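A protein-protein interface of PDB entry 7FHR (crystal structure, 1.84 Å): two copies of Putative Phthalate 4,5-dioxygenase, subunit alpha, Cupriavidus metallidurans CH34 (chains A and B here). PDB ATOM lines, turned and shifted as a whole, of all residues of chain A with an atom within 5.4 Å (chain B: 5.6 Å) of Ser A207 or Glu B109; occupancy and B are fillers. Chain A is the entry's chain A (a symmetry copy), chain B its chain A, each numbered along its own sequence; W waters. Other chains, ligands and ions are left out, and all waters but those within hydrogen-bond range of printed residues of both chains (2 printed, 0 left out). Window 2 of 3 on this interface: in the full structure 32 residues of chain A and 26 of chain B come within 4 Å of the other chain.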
ATOM      1  N   ASP A 205     -12.361 -31.671  19.790  1.00  0.00           N
ATOM      2  CA  ASP A 205     -11.069 -31.465  20.422  1.00  0.00           C
ATOM      3  C   ASP A 205     -11.316 -30.687  21.718  1.00  0.00           C
ATOM      4  O   ASP A 205     -11.714 -29.516  21.656  1.00  0.00           O
ATOM      5  CB  ASP A 205     -10.122 -30.733  19.465  1.00  0.00           C
ATOM      6  CG  ASP A 205      -8.721 -30.475  20.004  1.00  0.00           C
ATOM      7  OD1 ASP A 205      -8.460 -30.787  21.193  1.00  0.00           O
ATOM      8  OD2 ASP A 205      -7.885 -29.963  19.225  1.00  0.00           O
ATOM      9  N   LEU A 206     -11.128 -31.371  22.867  1.00  0.00           N
ATOM     10  CA  LEU A 206     -11.552 -30.863  24.171  1.00  0.00           C
ATOM     11  C   LEU A 206     -10.462 -29.995  24.776  1.00  0.00           C
ATOM     12  O   LEU A 206     -10.705 -29.320  25.780  1.00  0.00           O
ATOM     13  CB  LEU A 206     -11.864 -32.023  25.125  1.00  0.00           C
ATOM     14  CG  LEU A 206     -13.119 -32.819  24.785  1.00  0.00           C
ATOM     15  CD1 LEU A 206     -13.536 -33.682  25.973  1.00  0.00           C
ATOM     16  CD2 LEU A 206     -14.232 -31.873  24.360  1.00  0.00           C
ATOM     17  N   SER A 207      -9.260 -30.039  24.198  1.00  0.00           N
ATOM     18  CA  SER A 207      -8.184 -29.212  24.719  1.00  0.00           C
ATOM     19  C   SER A 207      -7.573 -28.350  23.625  1.00  0.00           C
ATOM     20  O   SER A 207      -6.447 -28.595  23.184  1.00  0.00           O
ATOM     21  CB  SER A 207      -7.155 -29.977  25.522  1.00  0.00           C
ATOM     22  OG  SER A 207      -6.921 -31.236  24.944  1.00  0.00           O
ATOM     23  N   PRO A 208      -8.245 -27.248  23.221  1.00  0.00           N
ATOM     24  CA  PRO A 208      -7.618 -26.300  22.303  1.00  0.00           C
ATOM     25  C   PRO A 208      -6.302 -25.800  22.901  1.00  0.00           C
ATOM     26  O   PRO A 208      -6.113 -25.840  24.126  1.00  0.00           O
ATOM     27  CB  PRO A 208      -8.687 -25.198  22.173  1.00  0.00           C
ATOM     28  CG  PRO A 208      -9.522 -25.309  23.435  1.00  0.00           C
ATOM     29  CD  PRO A 208      -9.586 -26.811  23.655  1.00  0.00           C
ATOM     30  N   THR A 209      -5.376 -25.404  22.010  1.00  0.00           N
ATOM     31  CA  THR A 209      -4.229 -24.580  22.354  1.00  0.00           C
ATOM     32  C   THR A 209      -4.652 -23.129  22.066  1.00  0.00           C
ATOM     33  O   THR A 209      -5.608 -22.922  21.290  1.00  0.00           O
ATOM     34  CB  THR A 209      -2.980 -25.037  21.568  1.00  0.00           C
ATOM     35  OG1 THR A 209      -3.259 -24.814  20.186  1.00  0.00           O
ATOM     36  CG2 THR A 209      -2.592 -26.480  21.818  1.00  0.00           C
ATOM     37  N   ARG A 224      -7.226 -22.946  19.106  1.00  0.00           N
ATOM     38  CA  ARG A 224      -6.934 -23.766  17.937  1.00  0.00           C
ATOM     39  C   ARG A 224      -7.233 -25.217  18.294  1.00  0.00           C
ATOM     40  O   ARG A 224      -6.690 -25.698  19.292  1.00  0.00           O
ATOM     41  CB  ARG A 224      -5.477 -23.568  17.520  1.00  0.00           C
ATOM     42  CG  ARG A 224      -5.049 -24.440  16.346  1.00  0.00           C
ATOM     43  CD  ARG A 224      -3.553 -24.299  16.166  1.00  0.00           C
ATOM     44  NE  ARG A 224      -3.072 -22.942  15.937  1.00  0.00           N
ATOM     45  CZ  ARG A 224      -2.980 -22.351  14.740  1.00  0.00           C
ATOM     46  NH1 ARG A 224      -3.338 -22.998  13.638  1.00  0.00           N
ATOM     47  NH2 ARG A 224      -2.515 -21.116  14.636  1.00  0.00           N
ATOM     48  N   GLY A 370      -5.314 -23.170  34.418  1.00  0.00           N
ATOM     49  CA  GLY A 370      -4.601 -24.079  33.522  1.00  0.00           C
ATOM     50  C   GLY A 370      -4.435 -23.446  32.146  1.00  0.00           C
ATOM     51  O   GLY A 370      -4.720 -22.254  31.978  1.00  0.00           O
ATOM     52  N   THR A 371      -3.991 -24.248  31.148  1.00  0.00           N
ATOM     53  CA  THR A 371      -3.835 -23.717  29.800  1.00  0.00           C
ATOM     54  C   THR A 371      -5.198 -23.304  29.247  1.00  0.00           C
ATOM     55  O   THR A 371      -5.258 -22.413  28.397  1.00  0.00           O
ATOM     56  CB  THR A 371      -3.036 -24.651  28.860  1.00  0.00           C
ATOM     57  OG1 THR A 371      -3.777 -25.864  28.764  1.00  0.00           O
ATOM     58  CG2 THR A 371      -1.690 -25.076  29.405  1.00  0.00           C
ATOM     59  N   SER A 372      -6.302 -23.920  29.713  1.00  0.00           N
ATOM     60  CA  SER A 372      -7.592 -23.540  29.163  1.00  0.00           C
ATOM     61  C   SER A 372      -7.959 -22.089  29.500  1.00  0.00           C
ATOM     62  O   SER A 372      -8.839 -21.534  28.849  1.00  0.00           O
ATOM     63  CB  SER A 372      -8.681 -24.456  29.630  1.00  0.00           C
ATOM     64  OG  SER A 372      -8.800 -24.370  31.040  1.00  0.00           O
ATOM     65  N   ASP A 373      -7.276 -21.478  30.492  1.00  0.00           N
ATOM     66  CA  ASP A 373      -7.509 -20.105  30.909  1.00  0.00           C
ATOM     67  C   ASP A 373      -6.540 -19.115  30.249  1.00  0.00           C
ATOM     68  O   ASP A 373      -6.481 -17.958  30.670  1.00  0.00           O
ATOM     69  CB  ASP A 373      -7.299 -19.992  32.424  1.00  0.00           C
ATOM     70  CG  ASP A 373      -8.241 -20.925  33.156  1.00  0.00           C
ATOM     71  OD1 ASP A 373      -9.465 -20.623  33.087  1.00  0.00           O
ATOM     72  OD2 ASP A 373      -7.753 -21.952  33.742  1.00  0.00           O
ATOM     73  N   TRP B  95     -12.947 -30.897  35.759  1.00  0.00           N
ATOM     74  CA  TRP B  95     -11.988 -31.432  36.727  1.00  0.00           C
ATOM     75  C   TRP B  95     -12.652 -32.486  37.598  1.00  0.00           C
ATOM     76  O   TRP B  95     -13.692 -32.225  38.184  1.00  0.00           O
ATOM     77  CB  TRP B  95     -11.341 -30.345  37.605  1.00  0.00           C
ATOM     78  CG  TRP B  95     -10.436 -29.410  36.882  1.00  0.00           C
ATOM     79  CD1 TRP B  95     -10.384 -29.141  35.542  1.00  0.00           C
ATOM     80  CD2 TRP B  95      -9.451 -28.578  37.500  1.00  0.00           C
ATOM     81  NE1 TRP B  95      -9.452 -28.167  35.285  1.00  0.00           N
ATOM     82  CE2 TRP B  95      -8.858 -27.805  36.472  1.00  0.00           C
ATOM     83  CE3 TRP B  95      -9.040 -28.391  38.827  1.00  0.00           C
ATOM     84  CZ2 TRP B  95      -7.831 -26.895  36.739  1.00  0.00           C
ATOM     85  CZ3 TRP B  95      -8.055 -27.458  39.084  1.00  0.00           C
ATOM     86  CH2 TRP B  95      -7.453 -26.728  38.057  1.00  0.00           C
ATOM     87  N   MET B 106      -8.310 -33.551  34.034  1.00  0.00           N
ATOM     88  CA  MET B 106      -8.598 -32.211  33.576  1.00  0.00           C
ATOM     89  C   MET B 106      -8.714 -32.268  32.051  1.00  0.00           C
ATOM     90  O   MET B 106      -7.752 -32.042  31.314  1.00  0.00           O
ATOM     91  CB  MET B 106      -7.500 -31.212  33.965  1.00  0.00           C
ATOM     92  CG  MET B 106      -7.113 -31.219  35.417  1.00  0.00           C
ATOM     93  SD  MET B 106      -5.708 -30.072  35.693  1.00  0.00           S
ATOM     94  CE  MET B 106      -5.759 -29.986  37.481  1.00  0.00           C
ATOM     95  N   PRO B 107      -9.922 -32.579  31.540  1.00  0.00           N
ATOM     96  CA  PRO B 107     -10.106 -32.850  30.111  1.00  0.00           C
ATOM     97  C   PRO B 107      -9.661 -31.701  29.213  1.00  0.00           C
ATOM     98  O   PRO B 107      -9.373 -31.914  28.035  1.00  0.00           O
ATOM     99  CB  PRO B 107     -11.632 -32.975  29.943  1.00  0.00           C
ATOM    100  CG  PRO B 107     -12.151 -33.304  31.352  1.00  0.00           C
ATOM    101  CD  PRO B 107     -11.162 -32.717  32.335  1.00  0.00           C
ATOM    102  N   CYS B 108      -9.618 -30.469  29.737  1.00  0.00           N
ATOM    103  CA  CYS B 108      -9.307 -29.409  28.798  1.00  0.00           C
ATOM    104  C   CYS B 108      -7.809 -29.187  28.704  1.00  0.00           C
ATOM    105  O   CYS B 108      -7.399 -28.311  27.936  1.00  0.00           O
ATOM    106  CB  CYS B 108      -9.944 -28.064  29.128  1.00  0.00           C
ATOM    107  SG  CYS B 108     -11.745 -28.125  29.264  1.00  0.00           S
ATOM    108  N   GLU B 109      -7.020 -29.919  29.500  1.00  0.00           N
ATOM    109  CA  GLU B 109      -5.589 -29.661  29.519  1.00  0.00           C
ATOM    110  C   GLU B 109      -4.860 -30.647  28.588  1.00  0.00           C
ATOM    111  O   GLU B 109      -5.347 -31.753  28.380  1.00  0.00           O
ATOM    112  CB  GLU B 109      -5.092 -29.758  30.962  1.00  0.00           C
ATOM    113  CG  GLU B 109      -5.705 -28.685  31.872  1.00  0.00           C
ATOM    114  CD  GLU B 109      -5.279 -27.280  31.480  1.00  0.00           C
ATOM    115  OE1 GLU B 109      -4.083 -27.107  31.155  1.00  0.00           O
ATOM    116  OE2 GLU B 109      -6.135 -26.373  31.435  1.00  0.00           O
ATOM    117  N   PRO B 110      -3.681 -30.309  28.000  1.00  0.00           N
ATOM    118  CA  PRO B 110      -2.871 -31.292  27.267  1.00  0.00           C
ATOM    119  C   PRO B 110      -2.772 -32.586  28.065  1.00  0.00           C
ATOM    120  O   PRO B 110      -2.811 -32.568  29.291  1.00  0.00           O
ATOM    121  CB  PRO B 110      -1.472 -30.643  27.245  1.00  0.00           C
ATOM    122  CG  PRO B 110      -1.759 -29.147  27.238  1.00  0.00           C
ATOM    123  CD  PRO B 110      -3.056 -28.971  28.016  1.00  0.00           C
ATOM    124  N   ALA B 111      -2.635 -33.719  27.374  1.00  0.00           N
ATOM    125  CA  ALA B 111      -2.650 -35.003  28.076  1.00  0.00           C
ATOM    126  C   ALA B 111      -1.304 -35.314  28.744  1.00  0.00           C
ATOM    127  O   ALA B 111      -1.229 -36.192  29.610  1.00  0.00           O
ATOM    128  CB  ALA B 111      -3.107 -36.133  27.170  1.00  0.00           C
ATOM    129  N   SER B 113       0.241 -33.020  30.502  1.00  0.00           N
ATOM    130  CA  SER B 113       0.343 -32.013  31.560  1.00  0.00           C
ATOM    131  C   SER B 113       0.448 -32.629  32.959  1.00  0.00           C
ATOM    132  O   SER B 113      -0.335 -33.501  33.304  1.00  0.00           O
ATOM    133  CB  SER B 113      -0.790 -31.016  31.458  1.00  0.00           C
ATOM    134  OG  SER B 113      -1.013 -30.366  32.703  1.00  0.00           O
ATOM    135  N   MET B 115      -0.004 -30.952  35.837  1.00  0.00           N
ATOM    136  CA  MET B 115      -0.861 -30.168  36.720  1.00  0.00           C
ATOM    137  C   MET B 115      -1.862 -31.090  37.417  1.00  0.00           C
ATOM    138  O   MET B 115      -2.045 -31.038  38.633  1.00  0.00           O
ATOM    139  CB  MET B 115      -1.602 -29.092  35.920  1.00  0.00           C
ATOM    140  CG  MET B 115      -2.284 -28.051  36.759  1.00  0.00           C
ATOM    141  SD  MET B 115      -3.216 -26.961  35.673  1.00  0.00           S
ATOM    142  CE  MET B 115      -1.979 -26.684  34.414  1.00  0.00           C
HETATM  143  O   HOH W   1      -7.763 -25.967  26.574  1.00  0.00           O
HETATM  144  O   HOH W   2      -8.581 -26.821  32.591  1.00  0.00           O
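Water W1 bridges the backbone carbonyl oxygen of Cys B108 and the backbone carbonyl oxygen of Pro A208.
Water W2 lies within hydrogen-bond range of OE2 of Glu B109 (2.7 Å), OG of Ser A372 (2.9 Å) and NE1 of Trp B95 (3.1 Å).
Among the printed residues, pairs that only touch across the chains: Leu A206 with Pro B107 (3.7 Å), Leu A206 with Cys B108 (3.3 Å), Ser A207 with Pro B107 (3.9 Å), Ser A207 with Cys B108 (2.9 Å), Ser A207 with Glu B109 (3.8 Å), Gly A370 with Glu B109 (3.5 Å), Gly A370 with Met B115 (3.8 Å), Thr A371 with Pro B110 (3.3 Å) and Ser A372 with Cys B108 (3.9 Å).
The side-chain carboxylate (OD1) of Asp A205 sits at hydrogen-bond distance from the backbone NH (N) of Ser A207 (3.2 Å).
OG of Ser B113 is in hydrogen-bond range of N of Met B115, at 3.3 Å.
The backbone NH (N) of Gly A370 lies within hydrogen-bond range of the side-chain carboxylate (OD2) of Asp A373 (2.8 Å).
Of the 9 printed residues of chain B, 5 touch a printed residue of chain A.
Hydrophobic or aromatic side chains of chain A within 4 Å of the printed part of chain B: Leu A206.
Along chain A the printed residues that touch a printed residue of chain B span positions 206 to 372.
Among the printed residues, 11 pairs touch across the chains.
Among the printed residues, no Asp or Glu carboxylate lies within 4 Å of a Lys or Arg side-chain nitrogen of the other chain.
No position is printed for both chains.
Of the 11 pairs that touch across the chains among the printed residues, none has its exchanged pair printed and touching as well.
Ser A207 touches just these residues of chain B: Pro B107, Cys B108 and Glu B109.
Of the printed residues of chain B, Thr A371 touches Glu B109 (2.7 Å) and Pro B110 (3.3 Å).
Of the printed residues of chain A, Pro B107 touches Leu A206 (3.7 Å) and Ser A207 (3.9 Å).
Printed residues of chain A within 4 Å of Met B115: Gly A370 (3.8 Å).
The nearest residue of chain B that does not touch Ser A207 is Pro B110 (4.3 Å).
The nearest printed residue of chain A that does not touch Cys B108 is Thr A371 (4.4 Å).
The side-chain carboxylate (OE1) of Glu B109 lies within hydrogen-bond range of the side-chain hydroxyl (OG1) of Thr A371 (2.7 Å).
The side-chain carboxylate (OE2) of Glu B109 is in hydrogen-bond range of the backbone NH (N) of Ser A372.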
